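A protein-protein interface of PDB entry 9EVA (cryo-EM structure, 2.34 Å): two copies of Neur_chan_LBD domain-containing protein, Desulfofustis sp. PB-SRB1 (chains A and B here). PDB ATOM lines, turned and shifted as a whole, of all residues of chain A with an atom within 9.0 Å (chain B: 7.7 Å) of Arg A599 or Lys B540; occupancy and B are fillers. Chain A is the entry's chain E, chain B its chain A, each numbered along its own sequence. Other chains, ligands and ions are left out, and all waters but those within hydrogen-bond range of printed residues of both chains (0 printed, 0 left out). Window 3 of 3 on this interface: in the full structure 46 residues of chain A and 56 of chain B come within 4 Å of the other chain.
Of the printed residues of chain B, Arg A599 touches Phe B538 and Lys B540. Lys B540 touches one residue of chain A. Of the printed residues of chain A, Phe B538 touches Arg A599 (3.7 Å). Printed residues of chain A within 4 Å of Leu B539: Lys A598 (3.98 Å). Printed residues of chain B within 4 Å of Leu A592: Val B535 (3.7 Å). The nearest residue of chain B that does not touch Arg A599 is Leu B539 (4.2 Å).
The backbone carbonyl oxygen (O) of Gly A543 lies within hydrogen-bond range of the guanidinium group (NH1) of Arg B544, 3.5 Å away.
O of Phe B538 sits at hydrogen-bond distance from NZ of Lys B540.
Among the printed residues, merely in contact across the chains: Leu A592 with Val B535, Lys A598 with Leu B539, Arg A599 with Phe B538 and Arg A599 with Lys B540.
4 positions are printed for both chains.
Of the 19 printed residues of chain A, 4 touch a printed residue of chain B. Hydrophobic or aromatic side chains of chain A within 4 Å of the printed part of chain B: Leu A592. Of the 18 printed residues of chain B, 5 touch a printed residue of chain A. Printed residues of chain B that touch a printed residue of chain A: Val B535, Phe B538, Leu B539, Lys B540 and Arg B544. Along chain B the printed residues that touch a printed residue of chain A span positions 535 to 544. Among the printed residues, 5 pairs touch across the chains. Among the printed residues, no Asp or Glu carboxylate lies within 4 Å of a Lys or Arg side-chain nitrogen of the other chain.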
ATOM      1  N   TYR A 542     -32.651  14.134  -8.409  1.00  0.00           N
ATOM      2  CA  TYR A 542     -32.571  12.685  -8.545  1.00  0.00           C
ATOM      3  C   TYR A 542     -31.170  12.135  -8.300  1.00  0.00           C
ATOM      4  O   TYR A 542     -31.036  10.947  -7.984  1.00  0.00           O
ATOM      5  CB  TYR A 542     -33.098  12.280  -9.921  1.00  0.00           C
ATOM      6  CG  TYR A 542     -34.557  12.643 -10.084  1.00  0.00           C
ATOM      7  CD1 TYR A 542     -35.543  11.929  -9.419  1.00  0.00           C
ATOM      8  CD2 TYR A 542     -34.946  13.713 -10.874  1.00  0.00           C
ATOM      9  CE1 TYR A 542     -36.874  12.262  -9.546  1.00  0.00           C
ATOM     10  CE2 TYR A 542     -36.279  14.053 -11.007  1.00  0.00           C
ATOM     11  CZ  TYR A 542     -37.237  13.324 -10.338  1.00  0.00           C
ATOM     12  OH  TYR A 542     -38.565  13.653 -10.465  1.00  0.00           O
ATOM     13  N   GLY A 543     -30.133  12.967  -8.408  1.00  0.00           N
ATOM     14  CA  GLY A 543     -28.800  12.514  -8.036  1.00  0.00           C
ATOM     15  C   GLY A 543     -28.687  12.211  -6.553  1.00  0.00           C
ATOM     16  O   GLY A 543     -28.116  11.189  -6.153  1.00  0.00           O
ATOM     17  N   LEU A 546     -30.535   8.969  -5.889  1.00  0.00           N
ATOM     18  CA  LEU A 546     -29.749   7.812  -6.301  1.00  0.00           C
ATOM     19  C   LEU A 546     -28.635   7.513  -5.303  1.00  0.00           C
ATOM     20  O   LEU A 546     -28.423   6.351  -4.926  1.00  0.00           O
ATOM     21  CB  LEU A 546     -29.179   8.053  -7.699  1.00  0.00           C
ATOM     22  CG  LEU A 546     -28.245   7.001  -8.297  1.00  0.00           C
ATOM     23  CD1 LEU A 546     -28.881   5.626  -8.231  1.00  0.00           C
ATOM     24  CD2 LEU A 546     -27.894   7.363  -9.729  1.00  0.00           C
ATOM     25  N   LEU A 592     -32.782   0.753  -8.844  1.00  0.00           N
ATOM     26  CA  LEU A 592     -33.042   0.682 -10.284  1.00  0.00           C
ATOM     27  C   LEU A 592     -33.988   1.797 -10.738  1.00  0.00           C
ATOM     28  O   LEU A 592     -33.741   2.470 -11.754  1.00  0.00           O
ATOM     29  CB  LEU A 592     -33.612  -0.689 -10.649  1.00  0.00           C
ATOM     30  CG  LEU A 592     -32.695  -1.901 -10.469  1.00  0.00           C
ATOM     31  CD1 LEU A 592     -33.466  -3.192 -10.679  1.00  0.00           C
ATOM     32  CD2 LEU A 592     -31.510  -1.828 -11.417  1.00  0.00           C
ATOM     33  N   ILE A 593     -35.068   2.017  -9.984  1.00  0.00           N
ATOM     34  CA  ILE A 593     -36.025   3.066 -10.328  1.00  0.00           C
ATOM     35  C   ILE A 593     -35.367   4.438 -10.245  1.00  0.00           C
ATOM     36  O   ILE A 593     -35.658   5.332 -11.049  1.00  0.00           O
ATOM     37  CB  ILE A 593     -37.270   2.973  -9.424  1.00  0.00           C
ATOM     38  CG1 ILE A 593     -38.010   1.658  -9.672  1.00  0.00           C
ATOM     39  CG2 ILE A 593     -38.199   4.154  -9.655  1.00  0.00           C
ATOM     40  CD1 ILE A 593     -39.208   1.457  -8.774  1.00  0.00           C
ATOM     41  N   SER A 594     -34.475   4.631  -9.269  1.00  0.00           N
ATOM     42  CA  SER A 594     -33.774   5.905  -9.154  1.00  0.00           C
ATOM     43  C   SER A 594     -32.908   6.174 -10.379  1.00  0.00           C
ATOM     44  O   SER A 594     -32.864   7.305 -10.881  1.00  0.00           O
ATOM     45  CB  SER A 594     -32.926   5.926  -7.883  1.00  0.00           C
ATOM     46  OG  SER A 594     -33.729   5.735  -6.733  1.00  0.00           O
ATOM     47  N   VAL A 595     -32.212   5.148 -10.876  1.00  0.00           N
ATOM     48  CA  VAL A 595     -31.410   5.324 -12.089  1.00  0.00           C
ATOM     49  C   VAL A 595     -32.302   5.696 -13.269  1.00  0.00           C
ATOM     50  O   VAL A 595     -31.975   6.593 -14.065  1.00  0.00           O
ATOM     51  CB  VAL A 595     -30.585   4.056 -12.383  1.00  0.00           C
ATOM     52  CG1 VAL A 595     -29.783   4.229 -13.660  1.00  0.00           C
ATOM     53  CG2 VAL A 595     -29.661   3.737 -11.223  1.00  0.00           C
ATOM     54  N   CYS A 596     -33.441   5.012 -13.402  1.00  0.00           N
ATOM     55  CA  CYS A 596     -34.355   5.319 -14.502  1.00  0.00           C
ATOM     56  C   CYS A 596     -34.859   6.759 -14.421  1.00  0.00           C
ATOM     57  O   CYS A 596     -34.929   7.466 -15.436  1.00  0.00           O
ATOM     58  CB  CYS A 596     -35.523   4.334 -14.499  1.00  0.00           C
ATOM     59  SG  CYS A 596     -36.744   4.628 -15.797  1.00  0.00           S
ATOM     60  N   GLN A 597     -35.216   7.210 -13.216  1.00  0.00           N
ATOM     61  CA  GLN A 597     -35.697   8.578 -13.044  1.00  0.00           C
ATOM     62  C   GLN A 597     -34.607   9.596 -13.352  1.00  0.00           C
ATOM     63  O   GLN A 597     -34.881  10.651 -13.934  1.00  0.00           O
ATOM     64  CB  GLN A 597     -36.224   8.776 -11.625  1.00  0.00           C
ATOM     65  CG  GLN A 597     -37.599   8.196 -11.395  1.00  0.00           C
ATOM     66  CD  GLN A 597     -38.084   8.406  -9.981  1.00  0.00           C
ATOM     67  OE1 GLN A 597     -37.297   8.404  -9.037  1.00  0.00           O
ATOM     68  NE2 GLN A 597     -39.384   8.598  -9.827  1.00  0.00           N
ATOM     69  N   LYS A 598     -33.366   9.307 -12.952  1.00  0.00           N
ATOM     70  CA  LYS A 598     -32.262  10.206 -13.274  1.00  0.00           C
ATOM     71  C   LYS A 598     -32.096  10.346 -14.780  1.00  0.00           C
ATOM     72  O   LYS A 598     -31.918  11.458 -15.296  1.00  0.00           O
ATOM     73  CB  LYS A 598     -30.970   9.699 -12.637  1.00  0.00           C
ATOM     74  CG  LYS A 598     -29.730  10.499 -12.994  1.00  0.00           C
ATOM     75  CD  LYS A 598     -29.761  11.880 -12.368  1.00  0.00           C
ATOM     76  CE  LYS A 598     -28.459  12.627 -12.605  1.00  0.00           C
ATOM     77  NZ  LYS A 598     -28.187  12.817 -14.055  1.00  0.00           N
ATOM     78  N   ARG A 599     -32.173   9.230 -15.508  1.00  0.00           N
ATOM     79  CA  ARG A 599     -32.062   9.313 -16.962  1.00  0.00           C
ATOM     80  C   ARG A 599     -33.218  10.111 -17.560  1.00  0.00           C
ATOM     81  O   ARG A 599     -33.010  10.966 -18.431  1.00  0.00           O
ATOM     82  CB  ARG A 599     -31.993   7.912 -17.571  1.00  0.00           C
ATOM     83  CG  ARG A 599     -31.774   7.915 -19.073  1.00  0.00           C
ATOM     84  CD  ARG A 599     -30.620   8.825 -19.462  1.00  0.00           C
ATOM     85  NE  ARG A 599     -30.540   9.012 -20.905  1.00  0.00           N
ATOM     86  CZ  ARG A 599     -29.773   9.913 -21.504  1.00  0.00           C
ATOM     87  NH1 ARG A 599     -29.000  10.732 -20.811  1.00  0.00           N
ATOM     88  NH2 ARG A 599     -29.785   9.996 -22.831  1.00  0.00           N
ATOM     89  N   LEU A 600     -34.446   9.855 -17.095  1.00  0.00           N
ATOM     90  CA  LEU A 600     -35.598  10.585 -17.622  1.00  0.00           C
ATOM     91  C   LEU A 600     -35.462  12.081 -17.379  1.00  0.00           C
ATOM     92  O   LEU A 600     -35.797  12.892 -18.250  1.00  0.00           O
ATOM     93  CB  LEU A 600     -36.893  10.060 -17.003  1.00  0.00           C
ATOM     94  CG  LEU A 600     -37.524   8.825 -17.642  1.00  0.00           C
ATOM     95  CD1 LEU A 600     -38.784   8.427 -16.896  1.00  0.00           C
ATOM     96  CD2 LEU A 600     -37.830   9.084 -19.102  1.00  0.00           C
ATOM     97  N   GLY A 601     -34.973  12.467 -16.200  1.00  0.00           N
ATOM     98  CA  GLY A 601     -34.718  13.874 -15.945  1.00  0.00           C
ATOM     99  C   GLY A 601     -33.642  14.441 -16.848  1.00  0.00           C
ATOM    100  O   GLY A 601     -33.709  15.602 -17.260  1.00  0.00           O
ATOM    101  N   ALA A 602     -32.632  13.630 -17.171  1.00  0.00           N
ATOM    102  CA  ALA A 602     -31.599  14.084 -18.097  1.00  0.00           C
ATOM    103  C   ALA A 602     -32.161  14.343 -19.492  1.00  0.00           C
ATOM    104  O   ALA A 602     -31.761  15.311 -20.148  1.00  0.00           O
ATOM    105  CB  ALA A 602     -30.465  13.062 -18.165  1.00  0.00           C
ATOM    106  N   VAL A 603     -33.087  13.500 -19.962  1.00  0.00           N
ATOM    107  CA  VAL A 603     -33.629  13.668 -21.313  1.00  0.00           C
ATOM    108  C   VAL A 603     -34.698  14.751 -21.393  1.00  0.00           C
ATOM    109  O   VAL A 603     -35.126  15.108 -22.497  1.00  0.00           O
ATOM    110  CB  VAL A 603     -34.168  12.316 -21.824  1.00  0.00           C
ATOM    111  CG1 VAL A 603     -34.419  12.346 -23.325  1.00  0.00           C
ATOM    112  CG2 VAL A 603     -33.186  11.205 -21.502  1.00  0.00           C
ATOM    113  N   GLY A 604     -35.125  15.309 -20.264  1.00  0.00           N
ATOM    114  CA  GLY A 604     -36.097  16.388 -20.294  1.00  0.00           C
ATOM    115  C   GLY A 604     -37.541  15.973 -20.124  1.00  0.00           C
ATOM    116  O   GLY A 604     -38.433  16.627 -20.673  1.00  0.00           O
ATOM    117  N   LYS A 605     -37.800  14.898 -19.383  1.00  0.00           N
ATOM    118  CA  LYS A 605     -39.144  14.386 -19.135  1.00  0.00           C
ATOM    119  C   LYS A 605     -39.485  14.401 -17.647  1.00  0.00           C
ATOM    120  O   LYS A 605     -39.945  13.403 -17.090  1.00  0.00           O
ATOM    121  CB  LYS A 605     -39.302  12.984 -19.715  1.00  0.00           C
ATOM    122  CG  LYS A 605     -39.200  12.929 -21.229  1.00  0.00           C
ATOM    123  CD  LYS A 605     -39.454  11.528 -21.755  1.00  0.00           C
ATOM    124  CE  LYS A 605     -39.333  11.489 -23.268  1.00  0.00           C
ATOM    125  NZ  LYS A 605     -39.585  10.130 -23.816  1.00  0.00           N
ATOM    126  N   GLN A 606     -39.236  15.534 -16.982  1.00  0.00           N
ATOM    127  CA  GLN A 606     -39.387  15.617 -15.530  1.00  0.00           C
ATOM    128  C   GLN A 606     -40.799  15.270 -15.065  1.00  0.00           C
ATOM    129  O   GLN A 606     -40.978  14.780 -13.943  1.00  0.00           O
ATOM    130  CB  GLN A 606     -39.010  17.016 -15.047  1.00  0.00           C
ATOM    131  CG  GLN A 606     -37.622  17.468 -15.456  1.00  0.00           C
ATOM    132  CD  GLN A 606     -37.296  18.859 -14.950  1.00  0.00           C
ATOM    133  OE1 GLN A 606     -38.145  19.534 -14.369  1.00  0.00           O
ATOM    134  NE2 GLN A 606     -36.060  19.294 -15.166  1.00  0.00           N
ATOM    135  N   ALA A 609     -41.031  11.612 -14.459  1.00  0.00           N
ATOM    136  CA  ALA A 609     -40.317  11.279 -13.231  1.00  0.00           C
ATOM    137  C   ALA A 609     -41.154  11.599 -11.998  1.00  0.00           C
ATOM    138  O   ALA A 609     -41.199  10.809 -11.046  1.00  0.00           O
ATOM    139  CB  ALA A 609     -38.981  12.020 -13.190  1.00  0.00           C
ATOM    140  N   VAL B 535     -27.461  -1.546 -15.518  1.00  0.00           N
ATOM    141  CA  VAL B 535     -28.381  -0.485 -15.928  1.00  0.00           C
ATOM    142  C   VAL B 535     -27.688   0.874 -16.014  1.00  0.00           C
ATOM    143  O   VAL B 535     -28.145   1.761 -16.743  1.00  0.00           O
ATOM    144  CB  VAL B 535     -29.593  -0.443 -14.975  1.00  0.00           C
ATOM    145  CG1 VAL B 535     -29.200   0.118 -13.620  1.00  0.00           C
ATOM    146  CG2 VAL B 535     -30.727   0.361 -15.584  1.00  0.00           C
ATOM    147  N   ILE B 536     -26.578   1.064 -15.295  1.00  0.00           N
ATOM    148  CA  ILE B 536     -25.973   2.390 -15.182  1.00  0.00           C
ATOM    149  C   ILE B 536     -25.387   2.891 -16.495  1.00  0.00           C
ATOM    150  O   ILE B 536     -25.082   4.081 -16.614  1.00  0.00           O
ATOM    151  CB  ILE B 536     -24.897   2.395 -14.077  1.00  0.00           C
ATOM    152  CG1 ILE B 536     -23.811   1.364 -14.384  1.00  0.00           C
ATOM    153  CG2 ILE B 536     -25.532   2.138 -12.724  1.00  0.00           C
ATOM    154  CD1 ILE B 536     -22.675   1.371 -13.396  1.00  0.00           C
ATOM    155  N   PHE B 537     -25.211   2.015 -17.486  1.00  0.00           N
ATOM    156  CA  PHE B 537     -24.618   2.436 -18.751  1.00  0.00           C
ATOM    157  C   PHE B 537     -25.569   3.253 -19.618  1.00  0.00           C
ATOM    158  O   PHE B 537     -25.133   3.783 -20.645  1.00  0.00           O
ATOM    159  CB  PHE B 537     -24.112   1.217 -19.520  1.00  0.00           C
ATOM    160  CG  PHE B 537     -22.787   0.707 -19.033  1.00  0.00           C
ATOM    161  CD1 PHE B 537     -22.710  -0.108 -17.918  1.00  0.00           C
ATOM    162  CD2 PHE B 537     -21.617   1.060 -19.679  1.00  0.00           C
ATOM    163  CE1 PHE B 537     -21.491  -0.569 -17.464  1.00  0.00           C
ATOM    164  CE2 PHE B 537     -20.396   0.601 -19.230  1.00  0.00           C
ATOM    165  CZ  PHE B 537     -20.333  -0.214 -18.121  1.00  0.00           C
ATOM    166  N   PHE B 538     -26.846   3.362 -19.245  1.00  0.00           N
ATOM    167  CA  PHE B 538     -27.744   4.269 -19.956  1.00  0.00           C
ATOM    168  C   PHE B 538     -27.437   5.729 -19.639  1.00  0.00           C
ATOM    169  O   PHE B 538     -27.776   6.615 -20.429  1.00  0.00           O
ATOM    170  CB  PHE B 538     -29.201   3.950 -19.617  1.00  0.00           C
ATOM    171  CG  PHE B 538     -29.726   2.715 -20.290  1.00  0.00           C
ATOM    172  CD1 PHE B 538     -30.135   2.752 -21.612  1.00  0.00           C
ATOM    173  CD2 PHE B 538     -29.820   1.520 -19.600  1.00  0.00           C
ATOM    174  CE1 PHE B 538     -30.621   1.620 -22.233  1.00  0.00           C
ATOM    175  CE2 PHE B 538     -30.305   0.385 -20.218  1.00  0.00           C
ATOM    176  CZ  PHE B 538     -30.705   0.436 -21.535  1.00  0.00           C
ATOM    177  N   LEU B 539     -26.812   5.997 -18.495  1.00  0.00           N
ATOM    178  CA  LEU B 539     -26.480   7.363 -18.116  1.00  0.00           C
ATOM    179  C   LEU B 539     -25.423   7.947 -19.046  1.00  0.00           C
ATOM    180  O   LEU B 539     -24.546   7.242 -19.552  1.00  0.00           O
ATOM    181  CB  LEU B 539     -25.975   7.407 -16.673  1.00  0.00           C
ATOM    182  CG  LEU B 539     -26.939   6.968 -15.571  1.00  0.00           C
ATOM    183  CD1 LEU B 539     -26.232   6.963 -14.227  1.00  0.00           C
ATOM    184  CD2 LEU B 539     -28.165   7.866 -15.536  1.00  0.00           C
ATOM    185  N   LYS B 540     -25.511   9.257 -19.266  1.00  0.00           N
ATOM    186  CA  LYS B 540     -24.525   9.986 -20.048  1.00  0.00           C
ATOM    187  C   LYS B 540     -23.640  10.882 -19.193  1.00  0.00           C
ATOM    188  O   LYS B 540     -22.726  11.520 -19.726  1.00  0.00           O
ATOM    189  CB  LYS B 540     -25.219  10.813 -21.136  1.00  0.00           C
ATOM    190  CG  LYS B 540     -25.870   9.968 -22.218  1.00  0.00           C
ATOM    191  CD  LYS B 540     -24.845   9.089 -22.911  1.00  0.00           C
ATOM    192  CE  LYS B 540     -25.502   8.130 -23.886  1.00  0.00           C
ATOM    193  NZ  LYS B 540     -26.368   7.141 -23.191  1.00  0.00           N
ATOM    194  N   ASP B 541     -23.887  10.951 -17.886  1.00  0.00           N
ATOM    195  CA  ASP B 541     -22.995  11.623 -16.942  1.00  0.00           C
ATOM    196  C   ASP B 541     -22.075  10.561 -16.352  1.00  0.00           C
ATOM    197  O   ASP B 541     -22.475   9.796 -15.471  1.00  0.00           O
ATOM    198  CB  ASP B 541     -23.794  12.341 -15.861  1.00  0.00           C
ATOM    199  CG  ASP B 541     -22.916  13.141 -14.916  1.00  0.00           C
ATOM    200  OD1 ASP B 541     -21.703  13.268 -15.180  1.00  0.00           O
ATOM    201  OD2 ASP B 541     -23.444  13.647 -13.904  1.00  0.00           O
ATOM    202  N   TYR B 542     -20.835  10.512 -16.839  1.00  0.00           N
ATOM    203  CA  TYR B 542     -19.953   9.397 -16.516  1.00  0.00           C
ATOM    204  C   TYR B 542     -19.415   9.451 -15.090  1.00  0.00           C
ATOM    205  O   TYR B 542     -19.000   8.411 -14.563  1.00  0.00           O
ATOM    206  CB  TYR B 542     -18.820   9.338 -17.541  1.00  0.00           C
ATOM    207  CG  TYR B 542     -19.338   9.076 -18.938  1.00  0.00           C
ATOM    208  CD1 TYR B 542     -19.855   7.835 -19.281  1.00  0.00           C
ATOM    209  CD2 TYR B 542     -19.335  10.070 -19.906  1.00  0.00           C
ATOM    210  CE1 TYR B 542     -20.345   7.588 -20.545  1.00  0.00           C
ATOM    211  CE2 TYR B 542     -19.823   9.831 -21.176  1.00  0.00           C
ATOM    212  CZ  TYR B 542     -20.327   8.587 -21.489  1.00  0.00           C
ATOM    213  OH  TYR B 542     -20.815   8.338 -22.749  1.00  0.00           O
ATOM    214  N   GLY B 543     -19.436  10.617 -14.444  1.00  0.00           N
ATOM    215  CA  GLY B 543     -19.065  10.673 -13.037  1.00  0.00           C
ATOM    216  C   GLY B 543     -20.043   9.923 -12.149  1.00  0.00           C
ATOM    217  O   GLY B 543     -19.641   9.168 -11.254  1.00  0.00           O
ATOM    218  N   ARG B 544     -21.342  10.119 -12.388  1.00  0.00           N
ATOM    219  CA  ARG B 544     -22.353   9.375 -11.645  1.00  0.00           C
ATOM    220  C   ARG B 544     -22.228   7.881 -11.899  1.00  0.00           C
ATOM    221  O   ARG B 544     -22.354   7.071 -10.972  1.00  0.00           O
ATOM    222  CB  ARG B 544     -23.752   9.861 -12.024  1.00  0.00           C
ATOM    223  CG  ARG B 544     -24.128  11.210 -11.450  1.00  0.00           C
ATOM    224  CD  ARG B 544     -24.342  11.130  -9.950  1.00  0.00           C
ATOM    225  NE  ARG B 544     -24.733  12.418  -9.391  1.00  0.00           N
ATOM    226  CZ  ARG B 544     -24.958  12.639  -8.104  1.00  0.00           C
ATOM    227  NH1 ARG B 544     -24.838  11.676  -7.206  1.00  0.00           N
ATOM    228  NH2 ARG B 544     -25.311  13.859  -7.707  1.00  0.00           N
ATOM    229  N   GLN B 545     -21.980   7.495 -13.152  1.00  0.00           N
ATOM    230  CA  GLN B 545     -21.810   6.084 -13.479  1.00  0.00           C
ATOM    231  C   GLN B 545     -20.623   5.491 -12.730  1.00  0.00           C
ATOM    232  O   GLN B 545     -20.712   4.392 -12.170  1.00  0.00           O
ATOM    233  CB  GLN B 545     -21.642   5.920 -14.990  1.00  0.00           C
ATOM    234  CG  GLN B 545     -21.325   4.502 -15.431  1.00  0.00           C
ATOM    235  CD  GLN B 545     -21.069   4.400 -16.919  1.00  0.00           C
ATOM    236  OE1 GLN B 545     -21.643   5.145 -17.711  1.00  0.00           O
ATOM    237  NE2 GLN B 545     -20.195   3.481 -17.308  1.00  0.00           N
ATOM    238  N   GLN B 606     -16.787  12.164 -26.799  1.00  0.00           N
ATOM    239  CA  GLN B 606     -18.011  11.593 -26.240  1.00  0.00           C
ATOM    240  C   GLN B 606     -18.648  10.550 -27.154  1.00  0.00           C
ATOM    241  O   GLN B 606     -19.348   9.650 -26.672  1.00  0.00           O
ATOM    242  CB  GLN B 606     -19.015  12.707 -25.946  1.00  0.00           C
ATOM    243  CG  GLN B 606     -18.485  13.798 -25.038  1.00  0.00           C
ATOM    244  CD  GLN B 606     -19.558  14.787 -24.635  1.00  0.00           C
ATOM    245  OE1 GLN B 606     -20.725  14.634 -24.994  1.00  0.00           O
ATOM    246  NE2 GLN B 606     -19.168  15.811 -23.884  1.00  0.00           N
ATOM    247  N   ALA B 609     -17.361   7.180 -26.302  1.00  0.00           N
ATOM    248  CA  ALA B 609     -17.946   6.740 -25.040  1.00  0.00           C
ATOM    249  C   ALA B 609     -19.361   6.209 -25.239  1.00  0.00           C
ATOM    250  O   ALA B 609     -19.736   5.183 -24.658  1.00  0.00           O
ATOM    251  CB  ALA B 609     -17.930   7.887 -24.031  1.00  0.00           C
ATOM    252  N   ALA B 610     -20.160   6.886 -26.069  1.00  0.00           N
ATOM    253  CA  ALA B 610     -21.503   6.390 -26.361  1.00  0.00           C
ATOM    254  C   ALA B 610     -21.468   5.044 -27.080  1.00  0.00           C
ATOM    255  O   ALA B 610     -22.273   4.148 -26.773  1.00  0.00           O
ATOM    256  CB  ALA B 610     -22.269   7.417 -27.193  1.00  0.00           C
ATOM    257  N   GLN B 611     -20.546   4.884 -28.031  1.00  0.00           N
ATOM    258  CA  GLN B 611     -20.406   3.601 -28.712  1.00  0.00           C
ATOM    259  C   GLN B 611     -20.012   2.491 -27.742  1.00  0.00           C
ATOM    260  O   GLN B 611     -20.530   1.368 -27.835  1.00  0.00           O
ATOM    261  CB  GLN B 611     -19.382   3.725 -29.840  1.00  0.00           C
ATOM    262  CG  GLN B 611     -19.379   2.574 -30.828  1.00  0.00           C
ATOM    263  CD  GLN B 611     -18.566   2.888 -32.068  1.00  0.00           C
ATOM    264  OE1 GLN B 611     -18.007   3.977 -32.196  1.00  0.00           O
ATOM    265  NE2 GLN B 611     -18.499   1.935 -32.992  1.00  0.00           N
ATOM    266  N   ASP B 613     -20.759   2.439 -24.572  1.00  0.00           N
ATOM    267  CA  ASP B 613     -21.962   2.164 -23.789  1.00  0.00           C
ATOM    268  C   ASP B 613     -22.878   1.184 -24.513  1.00  0.00           C
ATOM    269  O   ASP B 613     -23.360   0.208 -23.921  1.00  0.00           O
ATOM    270  CB  ASP B 613     -22.710   3.465 -23.488  1.00  0.00           C
ATOM    271  CG  ASP B 613     -22.038   4.291 -22.410  1.00  0.00           C
ATOM    272  OD1 ASP B 613     -21.339   3.707 -21.555  1.00  0.00           O
ATOM    273  OD2 ASP B 613     -22.213   5.527 -22.413  1.00  0.00           O
ATOM    274  N   THR B 614     -23.131   1.431 -25.803  1.00  0.00           N
ATOM    275  CA  THR B 614     -23.987   0.524 -26.563  1.00  0.00           C
ATOM    276  C   THR B 614     -23.388  -0.878 -26.627  1.00  0.00           C
ATOM    277  O   THR B 614     -24.099  -1.880 -26.447  1.00  0.00           O
ATOM    278  CB  THR B 614     -24.228   1.068 -27.972  1.00  0.00           C
ATOM    279  OG1 THR B 614     -22.980   1.195 -28.664  1.00  0.00           O
ATOM    280  CG2 THR B 614     -24.907   2.425 -27.912  1.00  0.00           C
ATOM    281  N   LEU B 617     -23.816  -2.632 -23.191  1.00  0.00           N
ATOM    282  CA  LEU B 617     -25.212  -2.992 -22.965  1.00  0.00           C
ATOM    283  C   LEU B 617     -25.623  -4.199 -23.794  1.00  0.00           C
ATOM    284  O   LEU B 617     -26.424  -5.020 -23.336  1.00  0.00           O
ATOM    285  CB  LEU B 617     -26.125  -1.807 -23.279  1.00  0.00           C
ATOM    286  CG  LEU B 617     -26.210  -0.689 -22.240  1.00  0.00           C
ATOM    287  CD1 LEU B 617     -26.957   0.503 -22.801  1.00  0.00           C
ATOM    288  CD2 LEU B 617     -26.873  -1.187 -20.970  1.00  0.00           C
